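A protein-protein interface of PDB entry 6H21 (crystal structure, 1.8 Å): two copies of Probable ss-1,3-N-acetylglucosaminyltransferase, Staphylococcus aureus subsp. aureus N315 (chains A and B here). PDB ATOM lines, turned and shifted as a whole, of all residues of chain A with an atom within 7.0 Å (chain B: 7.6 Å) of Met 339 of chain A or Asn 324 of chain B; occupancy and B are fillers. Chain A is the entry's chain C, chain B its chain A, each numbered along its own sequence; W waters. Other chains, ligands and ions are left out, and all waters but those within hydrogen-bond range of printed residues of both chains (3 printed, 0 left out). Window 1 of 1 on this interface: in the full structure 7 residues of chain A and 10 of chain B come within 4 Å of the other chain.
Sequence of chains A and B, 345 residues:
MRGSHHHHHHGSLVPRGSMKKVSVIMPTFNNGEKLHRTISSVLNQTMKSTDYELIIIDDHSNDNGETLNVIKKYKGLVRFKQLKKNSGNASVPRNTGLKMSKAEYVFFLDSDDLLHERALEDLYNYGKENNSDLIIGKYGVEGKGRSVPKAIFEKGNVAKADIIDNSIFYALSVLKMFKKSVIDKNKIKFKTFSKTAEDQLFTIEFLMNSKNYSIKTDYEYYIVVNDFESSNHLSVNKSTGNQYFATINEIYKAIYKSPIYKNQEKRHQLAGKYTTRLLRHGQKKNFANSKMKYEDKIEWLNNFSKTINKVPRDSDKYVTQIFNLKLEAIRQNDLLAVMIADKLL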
ATOM      1  N   PHE A 287      28.343 -12.006   9.283  1.00  0.00           N
ATOM      2  CA  PHE A 287      27.305 -12.623   8.469  1.00  0.00           C
ATOM      3  C   PHE A 287      26.073 -13.005   9.311  1.00  0.00           C
ATOM      4  O   PHE A 287      24.957 -12.992   8.801  1.00  0.00           O
ATOM      5  CB  PHE A 287      27.848 -13.872   7.770  1.00  0.00           C
ATOM      6  CG  PHE A 287      27.985 -15.085   8.655  1.00  0.00           C
ATOM      7  CD1 PHE A 287      29.105 -15.269   9.452  1.00  0.00           C
ATOM      8  CD2 PHE A 287      26.966 -16.025   8.719  1.00  0.00           C
ATOM      9  CE1 PHE A 287      29.215 -16.370  10.286  1.00  0.00           C
ATOM     10  CE2 PHE A 287      27.077 -17.122   9.557  1.00  0.00           C
ATOM     11  CZ  PHE A 287      28.202 -17.291  10.338  1.00  0.00           C
ATOM     12  N   ALA A 288      26.279 -13.385  10.574  1.00  0.00           N
ATOM     13  CA  ALA A 288      25.228 -14.109  11.360  1.00  0.00           C
ATOM     14  C   ALA A 288      23.958 -13.258  11.532  1.00  0.00           C
ATOM     15  O   ALA A 288      22.868 -13.799  11.409  1.00  0.00           O
ATOM     16  CB  ALA A 288      25.773 -14.609  12.688  1.00  0.00           C
ATOM     17  N   ASN A 289      24.095 -11.946  11.772  1.00  0.00           N
ATOM     18  CA  ASN A 289      22.952 -11.063  11.953  1.00  0.00           C
ATOM     19  C   ASN A 289      22.667 -10.234  10.683  1.00  0.00           C
ATOM     20  O   ASN A 289      21.955  -9.249  10.750  1.00  0.00           O
ATOM     21  CB  ASN A 289      23.166 -10.135  13.149  1.00  0.00           C
ATOM     22  CG  ASN A 289      23.162 -10.864  14.473  1.00  0.00           C
ATOM     23  OD1 ASN A 289      22.120 -11.329  14.930  1.00  0.00           O
ATOM     24  ND2 ASN A 289      24.308 -10.944  15.109  1.00  0.00           N
ATOM     25  N   SER A 290      23.254 -10.630   9.542  1.00  0.00           N
ATOM     26  CA  SER A 290      23.154  -9.916   8.284  1.00  0.00           C
ATOM     27  C   SER A 290      21.817 -10.234   7.614  1.00  0.00           C
ATOM     28  O   SER A 290      21.041 -11.050   8.095  1.00  0.00           O
ATOM     29  CB  SER A 290      24.315 -10.268   7.363  1.00  0.00           C
ATOM     30  OG  SER A 290      24.135 -11.552   6.762  1.00  0.00           O
ATOM     31  N   LYS A 297      23.455 -18.580   5.260  1.00  0.00           N
ATOM     32  CA  LYS A 297      24.162 -18.467   6.541  1.00  0.00           C
ATOM     33  C   LYS A 297      24.598 -19.859   7.013  1.00  0.00           C
ATOM     34  O   LYS A 297      25.710 -20.036   7.495  1.00  0.00           O
ATOM     35  CB  LYS A 297      23.281 -17.829   7.617  1.00  0.00           C
ATOM     36  CG  LYS A 297      22.916 -16.379   7.373  1.00  0.00           C
ATOM     37  CD  LYS A 297      22.031 -15.788   8.460  1.00  0.00           C
ATOM     38  CE  LYS A 297      22.031 -14.278   8.396  1.00  0.00           C
ATOM     39  NZ  LYS A 297      21.011 -13.689   9.282  1.00  0.00           N
ATOM     40  N   ALA A 329      31.281 -20.802  19.286  1.00  0.00           N
ATOM     41  CA  ALA A 329      30.043 -20.947  18.563  1.00  0.00           C
ATOM     42  C   ALA A 329      30.322 -21.438  17.132  1.00  0.00           C
ATOM     43  O   ALA A 329      29.595 -22.280  16.631  1.00  0.00           O
ATOM     44  CB  ALA A 329      29.277 -19.656  18.576  1.00  0.00           C
ATOM     45  N   ASP A 334      26.904 -23.440  15.395  1.00  0.00           N
ATOM     46  CA  ASP A 334      25.665 -23.046  16.066  1.00  0.00           C
ATOM     47  C   ASP A 334      25.324 -21.602  15.692  1.00  0.00           C
ATOM     48  O   ASP A 334      25.869 -20.666  16.264  1.00  0.00           O
ATOM     49  CB  ASP A 334      25.807 -23.207  17.580  1.00  0.00           C
ATOM     50  CG  ASP A 334      24.509 -23.109  18.378  1.00  0.00           C
ATOM     51  OD1 ASP A 334      23.720 -22.152  18.183  1.00  0.00           O
ATOM     52  OD2 ASP A 334      24.359 -23.933  19.285  1.00  0.00           O
ATOM     53  N   LEU A 335      24.440 -21.440  14.701  1.00  0.00           N
ATOM     54  CA  LEU A 335      24.185 -20.151  14.129  1.00  0.00           C
ATOM     55  C   LEU A 335      23.587 -19.223  15.196  1.00  0.00           C
ATOM     56  O   LEU A 335      23.946 -18.063  15.245  1.00  0.00           O
ATOM     57  CB  LEU A 335      23.270 -20.289  12.909  1.00  0.00           C
ATOM     58  CG  LEU A 335      22.863 -18.962  12.266  1.00  0.00           C
ATOM     59  CD1 LEU A 335      24.075 -18.199  11.749  1.00  0.00           C
ATOM     60  CD2 LEU A 335      21.846 -19.171  11.147  1.00  0.00           C
ATOM     61  N   LEU A 336      22.695 -19.750  16.049  1.00  0.00           N
ATOM     62  CA  LEU A 336      22.045 -18.923  17.127  1.00  0.00           C
ATOM     63  C   LEU A 336      23.117 -18.340  18.056  1.00  0.00           C
ATOM     64  O   LEU A 336      23.050 -17.177  18.463  1.00  0.00           O
ATOM     65  CB  LEU A 336      21.044 -19.774  17.918  1.00  0.00           C
ATOM     66  CG  LEU A 336      19.694 -20.049  17.249  1.00  0.00           C
ATOM     67  CD1 LEU A 336      18.815 -20.934  18.116  1.00  0.00           C
ATOM     68  CD2 LEU A 336      18.958 -18.767  16.950  1.00  0.00           C
ATOM     69  N   ALA A 337      24.086 -19.181  18.399  1.00  0.00           N
ATOM     70  CA  ALA A 337      25.187 -18.804  19.281  1.00  0.00           C
ATOM     71  C   ALA A 337      26.089 -17.767  18.603  1.00  0.00           C
ATOM     72  O   ALA A 337      26.537 -16.856  19.261  1.00  0.00           O
ATOM     73  CB  ALA A 337      25.954 -20.019  19.712  1.00  0.00           C
ATOM     74  N   VAL A 338      26.310 -17.856  17.284  1.00  0.00           N
ATOM     75  CA  VAL A 338      27.120 -16.820  16.604  1.00  0.00           C
ATOM     76  C   VAL A 338      26.367 -15.481  16.615  1.00  0.00           C
ATOM     77  O   VAL A 338      26.947 -14.427  16.922  1.00  0.00           O
ATOM     78  CB  VAL A 338      27.561 -17.240  15.187  1.00  0.00           C
ATOM     79  CG1 VAL A 338      28.406 -16.158  14.530  1.00  0.00           C
ATOM     80  CG2 VAL A 338      28.308 -18.567  15.206  1.00  0.00           C
ATOM     81  N   MET A 339      25.072 -15.527  16.283  1.00  0.00           N
ATOM     82  CA  MET A 339      24.207 -14.374  16.331  1.00  0.00           C
ATOM     83  C   MET A 339      24.301 -13.713  17.721  1.00  0.00           C
ATOM     84  O   MET A 339      24.482 -12.505  17.817  1.00  0.00           O
ATOM     85  CB  MET A 339      22.756 -14.765  16.048  1.00  0.00           C
ATOM     86  CG  MET A 339      22.494 -15.126  14.603  1.00  0.00           C
ATOM     87  SD  MET A 339      20.816 -15.710  14.373  1.00  0.00           S
ATOM     88  CE  MET A 339      19.884 -14.185  14.411  1.00  0.00           C
ATOM     89  N   ILE A 340      24.203 -14.517  18.773  1.00  0.00           N
ATOM     90  CA  ILE A 340      24.254 -13.997  20.149  1.00  0.00           C
ATOM     91  C   ILE A 340      25.650 -13.415  20.412  1.00  0.00           C
ATOM     92  O   ILE A 340      25.766 -12.320  20.865  1.00  0.00           O
ATOM     93  CB  ILE A 340      23.866 -15.088  21.160  1.00  0.00           C
ATOM     94  CG1 ILE A 340      22.381 -15.453  21.049  1.00  0.00           C
ATOM     95  CG2 ILE A 340      24.227 -14.670  22.575  1.00  0.00           C
ATOM     96  CD1 ILE A 340      22.062 -16.838  21.581  1.00  0.00           C
ATOM     97  N   ALA A 341      26.699 -14.142  20.027  1.00  0.00           N
ATOM     98  CA  ALA A 341      28.088 -13.663  20.235  1.00  0.00           C
ATOM     99  C   ALA A 341      28.277 -12.283  19.594  1.00  0.00           C
ATOM    100  O   ALA A 341      28.880 -11.380  20.206  1.00  0.00           O
ATOM    101  CB  ALA A 341      29.078 -14.651  19.684  1.00  0.00           C
ATOM    102  N   ASP A 342      27.699 -12.092  18.396  1.00  0.00           N
ATOM    103  CA  ASP A 342      27.865 -10.833  17.661  1.00  0.00           C
ATOM    104  C   ASP A 342      27.102  -9.695  18.351  1.00  0.00           C
ATOM    105  O   ASP A 342      27.590  -8.571  18.350  1.00  0.00           O
ATOM    106  CB  ASP A 342      27.445 -10.964  16.198  1.00  0.00           C
ATOM    107  CG  ASP A 342      28.551 -11.473  15.293  1.00  0.00           C
ATOM    108  OD1 ASP A 342      29.754 -11.414  15.702  1.00  0.00           O
ATOM    109  OD2 ASP A 342      28.227 -11.912  14.176  1.00  0.00           O
ATOM    110  N   LYS A 343      25.920  -9.986  18.915  1.00  0.00           N
ATOM    111  CA  LYS A 343      25.153  -8.988  19.692  1.00  0.00           C
ATOM    112  C   LYS A 343      25.912  -8.542  20.949  1.00  0.00           C
ATOM    113  O   LYS A 343      25.698  -7.399  21.420  1.00  0.00           O
ATOM    114  CB  LYS A 343      23.773  -9.525  20.082  1.00  0.00           C
ATOM    115  CG  LYS A 343      22.709  -9.304  19.020  1.00  0.00           C
ATOM    116  CD  LYS A 343      21.462 -10.109  19.246  1.00  0.00           C
ATOM    117  CE  LYS A 343      20.669 -10.276  17.964  1.00  0.00           C
ATOM    118  NZ  LYS A 343      20.341  -8.972  17.344  1.00  0.00           N
ATOM    119  N   LEU A 344      26.737  -9.432  21.526  1.00  0.00           N
ATOM    120  CA  LEU A 344      27.466  -9.122  22.759  1.00  0.00           C
ATOM    121  C   LEU A 344      28.793  -8.397  22.487  1.00  0.00           C
ATOM    122  O   LEU A 344      29.273  -7.691  23.355  1.00  0.00           O
ATOM    123  CB  LEU A 344      27.672 -10.408  23.555  1.00  0.00           C
ATOM    124  CG  LEU A 344      26.398 -11.003  24.140  1.00  0.00           C
ATOM    125  CD1 LEU A 344      26.678 -12.349  24.781  1.00  0.00           C
ATOM    126  CD2 LEU A 344      25.739 -10.060  25.138  1.00  0.00           C
ATOM    127  N   LEU B 279       5.140 -10.538  18.028  1.00  0.00           N
ATOM    128  CA  LEU B 279       6.287 -10.479  18.900  1.00  0.00           C
ATOM    129  C   LEU B 279       6.224  -9.262  19.827  1.00  0.00           C
ATOM    130  O   LEU B 279       6.689  -9.329  20.951  1.00  0.00           O
ATOM    131  CB  LEU B 279       7.540 -10.463  18.025  1.00  0.00           C
ATOM    132  CG  LEU B 279       7.810 -11.796  17.340  1.00  0.00           C
ATOM    133  CD1 LEU B 279       9.001 -11.688  16.391  1.00  0.00           C
ATOM    134  CD2 LEU B 279       8.031 -12.879  18.380  1.00  0.00           C
ATOM    135  N   ASP B 316      10.283 -13.221   6.663  1.00  0.00           N
ATOM    136  CA  ASP B 316      11.152 -12.842   7.778  1.00  0.00           C
ATOM    137  C   ASP B 316      11.840 -11.492   7.521  1.00  0.00           C
ATOM    138  O   ASP B 316      12.025 -10.722   8.464  1.00  0.00           O
ATOM    139  CB  ASP B 316      12.146 -13.964   8.103  1.00  0.00           C
ATOM    140  CG  ASP B 316      11.500 -15.187   8.743  1.00  0.00           C
ATOM    141  OD1 ASP B 316      10.247 -15.164   8.940  1.00  0.00           O
ATOM    142  OD2 ASP B 316      12.235 -16.160   9.037  1.00  0.00           O
ATOM    143  N   VAL B 319      10.192  -8.425   9.047  1.00  0.00           N
ATOM    144  CA  VAL B 319      10.112  -8.330  10.489  1.00  0.00           C
ATOM    145  C   VAL B 319      11.152  -7.317  10.981  1.00  0.00           C
ATOM    146  O   VAL B 319      12.270  -7.303  10.485  1.00  0.00           O
ATOM    147  CB  VAL B 319      10.312  -9.704  11.152  1.00  0.00           C
ATOM    148  CG1 VAL B 319      10.409  -9.586  12.665  1.00  0.00           C
ATOM    149  CG2 VAL B 319       9.218 -10.690  10.761  1.00  0.00           C
ATOM    150  N   THR B 320      10.780  -6.489  11.970  1.00  0.00           N
ATOM    151  CA  THR B 320      11.705  -5.507  12.564  1.00  0.00           C
ATOM    152  C   THR B 320      13.002  -6.219  13.000  1.00  0.00           C
ATOM    153  O   THR B 320      12.958  -7.244  13.668  1.00  0.00           O
ATOM    154  CB  THR B 320      11.041  -4.721  13.706  1.00  0.00           C
ATOM    155  OG1 THR B 320       9.786  -4.187  13.277  1.00  0.00           O
ATOM    156  CG2 THR B 320      11.866  -3.542  14.163  1.00  0.00           C
ATOM    157  N   GLN B 321      14.150  -5.647  12.626  1.00  0.00           N
ATOM    158  CA  GLN B 321      15.479  -6.312  12.755  1.00  0.00           C
ATOM    159  C   GLN B 321      15.824  -6.646  14.217  1.00  0.00           C
ATOM    160  O   GLN B 321      16.557  -7.610  14.454  1.00  0.00           O
ATOM    161  CB  GLN B 321      16.603  -5.458  12.164  1.00  0.00           C
ATOM    162  CG  GLN B 321      16.542  -5.287  10.647  1.00  0.00           C
ATOM    163  N   ILE B 322      15.288  -5.905  15.203  1.00  0.00           N
ATOM    164  CA  ILE B 322      15.597  -6.232  16.622  1.00  0.00           C
ATOM    165  C   ILE B 322      15.071  -7.609  17.001  1.00  0.00           C
ATOM    166  O   ILE B 322      15.590  -8.175  17.931  1.00  0.00           O
ATOM    167  CB  ILE B 322      15.090  -5.209  17.654  1.00  0.00           C
ATOM    168  CG1 ILE B 322      13.633  -4.813  17.422  1.00  0.00           C
ATOM    169  CG2 ILE B 322      16.036  -4.022  17.707  1.00  0.00           C
ATOM    170  CD1 ILE B 322      12.925  -4.329  18.674  1.00  0.00           C
ATOM    171  N   PHE B 323      14.059  -8.114  16.292  1.00  0.00           N
ATOM    172  CA  PHE B 323      13.476  -9.406  16.578  1.00  0.00           C
ATOM    173  C   PHE B 323      14.148 -10.565  15.821  1.00  0.00           C
ATOM    174  O   PHE B 323      13.682 -11.693  15.950  1.00  0.00           O
ATOM    175  CB  PHE B 323      11.982  -9.387  16.251  1.00  0.00           C
ATOM    176  CG  PHE B 323      11.195  -8.465  17.148  1.00  0.00           C
ATOM    177  CD1 PHE B 323      11.203  -8.649  18.521  1.00  0.00           C
ATOM    178  CD2 PHE B 323      10.483  -7.397  16.627  1.00  0.00           C
ATOM    179  CE1 PHE B 323      10.479  -7.813  19.356  1.00  0.00           C
ATOM    180  CE2 PHE B 323       9.774  -6.547  17.466  1.00  0.00           C
ATOM    181  CZ  PHE B 323       9.774  -6.755  18.827  1.00  0.00           C
ATOM    182  N   ASN B 324      15.231 -10.304  15.075  1.00  0.00           N
ATOM    183  CA  ASN B 324      15.882 -11.325  14.233  1.00  0.00           C
ATOM    184  C   ASN B 324      16.213 -12.583  15.057  1.00  0.00           C
ATOM    185  O   ASN B 324      15.857 -13.713  14.678  1.00  0.00           O
ATOM    186  CB  ASN B 324      17.112 -10.763  13.502  1.00  0.00           C
ATOM    187  CG  ASN B 324      18.305 -10.422  14.380  1.00  0.00           C
ATOM    188  OD1 ASN B 324      18.178 -10.078  15.570  1.00  0.00           O
ATOM    189  ND2 ASN B 324      19.498 -10.550  13.813  1.00  0.00           N
ATOM    190  N   LEU B 325      16.856 -12.398  16.211  1.00  0.00           N
ATOM    191  CA  LEU B 325      17.314 -13.526  16.999  1.00  0.00           C
ATOM    192  C   LEU B 325      16.125 -14.259  17.638  1.00  0.00           C
ATOM    193  O   LEU B 325      16.060 -15.496  17.615  1.00  0.00           O
ATOM    194  CB  LEU B 325      18.316 -13.060  18.052  1.00  0.00           C
ATOM    195  CG  LEU B 325      18.711 -14.123  19.074  1.00  0.00           C
ATOM    196  CD1 LEU B 325      19.428 -15.297  18.412  1.00  0.00           C
ATOM    197  CD2 LEU B 325      19.557 -13.506  20.178  1.00  0.00           C
ATOM    198  N   LYS B 326      15.181 -13.501  18.205  1.00  0.00           N
ATOM    199  CA  LYS B 326      14.063 -14.105  18.854  1.00  0.00           C
ATOM    200  C   LYS B 326      13.291 -14.974  17.849  1.00  0.00           C
ATOM    201  O   LYS B 326      12.909 -16.093  18.167  1.00  0.00           O
ATOM    202  CB  LYS B 326      13.153 -13.041  19.486  1.00  0.00           C
ATOM    203  CG  LYS B 326      11.978 -13.615  20.267  1.00  0.00           C
ATOM    204  CD  LYS B 326      11.482 -12.738  21.371  1.00  0.00           C
ATOM    205  CE  LYS B 326      10.423 -13.420  22.209  1.00  0.00           C
ATOM    206  NZ  LYS B 326       9.775 -12.433  23.117  1.00  0.00           N
ATOM    207  N   LEU B 327      13.029 -14.417  16.661  1.00  0.00           N
ATOM    208  CA  LEU B 327      12.250 -15.105  15.623  1.00  0.00           C
ATOM    209  C   LEU B 327      12.975 -16.401  15.212  1.00  0.00           C
ATOM    210  O   LEU B 327      12.358 -17.447  15.159  1.00  0.00           O
ATOM    211  CB  LEU B 327      12.029 -14.186  14.417  1.00  0.00           C
ATOM    212  CG  LEU B 327      11.261 -14.833  13.263  1.00  0.00           C
ATOM    213  CD1 LEU B 327       9.901 -15.313  13.734  1.00  0.00           C
ATOM    214  CD2 LEU B 327      11.115 -13.883  12.087  1.00  0.00           C
ATOM    215  N   GLU B 328      14.289 -16.327  15.000  1.00  0.00           N
ATOM    216  CA  GLU B 328      15.074 -17.534  14.623  1.00  0.00           C
ATOM    217  C   GLU B 328      15.036 -18.575  15.754  1.00  0.00           C
ATOM    218  O   GLU B 328      14.861 -19.756  15.488  1.00  0.00           O
ATOM    219  CB  GLU B 328      16.509 -17.184  14.226  1.00  0.00           C
ATOM    220  CG  GLU B 328      17.223 -18.326  13.499  1.00  0.00           C
ATOM    221  CD  GLU B 328      16.448 -18.873  12.305  1.00  0.00           C
ATOM    222  OE1 GLU B 328      16.055 -18.061  11.428  1.00  0.00           O
ATOM    223  OE2 GLU B 328      16.197 -20.090  12.266  1.00  0.00           O
ATOM    224  N   ALA B 329      15.144 -18.124  17.014  1.00  0.00           N
ATOM    225  CA  ALA B 329      15.120 -19.011  18.178  1.00  0.00           C
ATOM    226  C   ALA B 329      13.804 -19.801  18.211  1.00  0.00           C
ATOM    227  O   ALA B 329      13.812 -20.997  18.469  1.00  0.00           O
ATOM    228  CB  ALA B 329      15.346 -18.231  19.453  1.00  0.00           C
ATOM    229  N   ILE B 330      12.692 -19.104  17.940  1.00  0.00           N
ATOM    230  CA  ILE B 330      11.390 -19.723  17.866  1.00  0.00           C
ATOM    231  C   ILE B 330      11.344 -20.736  16.707  1.00  0.00           C
ATOM    232  O   ILE B 330      10.871 -21.827  16.905  1.00  0.00           O
ATOM    233  CB  ILE B 330      10.270 -18.668  17.742  1.00  0.00           C
ATOM    234  CG1 ILE B 330      10.199 -17.786  18.988  1.00  0.00           C
ATOM    235  CG2 ILE B 330       8.943 -19.340  17.443  1.00  0.00           C
ATOM    236  CD1 ILE B 330       9.448 -16.483  18.776  1.00  0.00           C
ATOM    237  N   ALA B 341      17.412 -14.252  23.948  1.00  0.00           N
ATOM    238  CA  ALA B 341      16.921 -13.226  23.064  1.00  0.00           C
ATOM    239  C   ALA B 341      16.162 -12.163  23.881  1.00  0.00           C
ATOM    240  O   ALA B 341      16.346 -10.973  23.676  1.00  0.00           O
ATOM    241  CB  ALA B 341      16.042 -13.830  21.994  1.00  0.00           C
ATOM    242  N   LEU B 344      18.303  -9.782  25.827  1.00  0.00           N
ATOM    243  CA  LEU B 344      19.021  -8.788  25.011  1.00  0.00           C
ATOM    244  C   LEU B 344      18.058  -7.768  24.392  1.00  0.00           C
ATOM    245  O   LEU B 344      18.505  -6.853  23.725  1.00  0.00           O
ATOM    246  CB  LEU B 344      19.827  -9.479  23.900  1.00  0.00           C
ATOM    247  CG  LEU B 344      20.867 -10.503  24.347  1.00  0.00           C
ATOM    248  CD1 LEU B 344      21.416 -11.259  23.153  1.00  0.00           C
ATOM    249  CD2 LEU B 344      21.997  -9.839  25.097  1.00  0.00           C
ATOM    250  N   LEU B 345      16.754  -7.949  24.576  1.00  0.00           N
ATOM    251  CA  LEU B 345      15.751  -6.956  24.183  1.00  0.00           C
ATOM    252  C   LEU B 345      15.402  -6.066  25.393  1.00  0.00           C
ATOM    253  O   LEU B 345      16.046  -6.076  26.460  1.00  0.00           O
ATOM    254  CB  LEU B 345      14.505  -7.685  23.666  1.00  0.00           C
ATOM    255  CG  LEU B 345      14.671  -8.387  22.320  1.00  0.00           C
ATOM    256  CD1 LEU B 345      13.503  -9.323  22.069  1.00  0.00           C
ATOM    257  CD2 LEU B 345      14.797  -7.373  21.196  1.00  0.00           C
ATOM    258  OXT LEU B 345      14.421  -5.318  25.345  1.00  0.00           O
HETATM  259  O   HOH W   1      18.023  -8.054  19.293  1.00  0.00           O
HETATM  260  O   HOH W   2      19.086  -7.081  15.044  1.00  0.00           O
HETATM  261  O   HOH W   3      19.427 -12.143  11.273  1.00  0.00           O
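Leu 344 of chain A touches its own counterpart, Leu 344 of chain B. Positions printed for both chains: 329, 341 and 344. Of the 10 pairs that touch across the chains among the printed residues, 1 has its exchanged pair printed and touching as well.
The side-chain amide oxygen of Asn 324 of chain B lies close to the backbone carbonyl oxygen of Gln 321 of chain B, 3.2 Å away. The backbone carbonyl oxygen (O) of Met 339 of chain A lies within hydrogen-bond range of the side-chain amide nitrogen (ND2) of Asn 289 of chain A (3.1 Å). OD1 of Asp 334 of chain A sits close to N of Leu 336 of chain A (3.4 Å).
Of the 17 printed residues of chain B, 5 touch a printed residue of chain A. Hydrophobic or aromatic side chains of chain B within 4 Å of the printed part of chain A: Leu 325 and Leu 344. Hydrophobic or aromatic side chains of chain A that line the printed part of chain B: Leu 336, Met 339, Ile 340 and Leu 344.
Of the printed residues of chain B, Leu 336 of chain A touches Leu 325 (3.8 Å), Glu 328 (3.9 Å) and Ala 329 (3.9 Å). Of chain B, only Asn 324 (3.7 Å) and Leu 325 (3.7 Å) come within 4 Å of Met 339 of chain A. Of the printed residues of chain B, Ile 340 of chain A touches Leu 325. Of the printed residues of chain A, Asn 324 of chain B touches Asn 289, Met 339 and Lys 343. Of the printed residues of chain A, Leu 325 of chain B touches Leu 336, Met 339, Ile 340 and Lys 343. Of the printed residues of chain A, Glu 328 of chain B touches Leu 336. The nearest residue of chain B that does not touch Met 339 of chain A is Glu 328 of chain B (4.5 Å). The nearest residue of chain A that does not touch Asn 324 of chain B is Ala 288 of chain A (5.3 Å). The nearest printed residue of chain B that does not touch Asn 289 of chain A is Leu 325 of chain B (5.2 Å).
Water W2 lies within hydrogen-bond range of O of Gln 321 of chain B, OD1 of Asn 324 of chain B and NZ of Lys 343 of chain A. Water W1 lies within hydrogen-bond range of O of Ile 322 of chain B and NZ of Lys 343 of chain A. Water W3 bridges NZ of Lys 297 of chain A (3.0 Å) and ND2 of Asn 324 of chain B (3.0 Å).
OD1 of Asn 289 of chain A lies within hydrogen-bond range of ND2 of Asn 324 of chain B, 3.0 Å away. The side-chain amide oxygen (OD1) of Asn 324 of chain B sits at hydrogen-bond distance from the side-chain amino group (NZ) of Lys 343 of chain A, 3.0 Å away.
Among the printed residues, merely in contact across the chains: Leu 336 of chain A with Leu 325 of chain B (3.8 Å), Leu 336 of chain A with Glu 328 of chain B (3.9 Å), Leu 336 of chain A with Ala 329 of chain B (3.9 Å), Met 339 of chain A with Asn 324 of chain B (3.7 Å), Met 339 of chain A with Leu 325 of chain B (3.7 Å), Ile 340 of chain A with Leu 325 of chain B (3.5 Å), Lys 343 of chain A with Leu 325 of chain B (3.6 Å) and Leu 344 of chain A with Leu 344 of chain B (3.7 Å).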
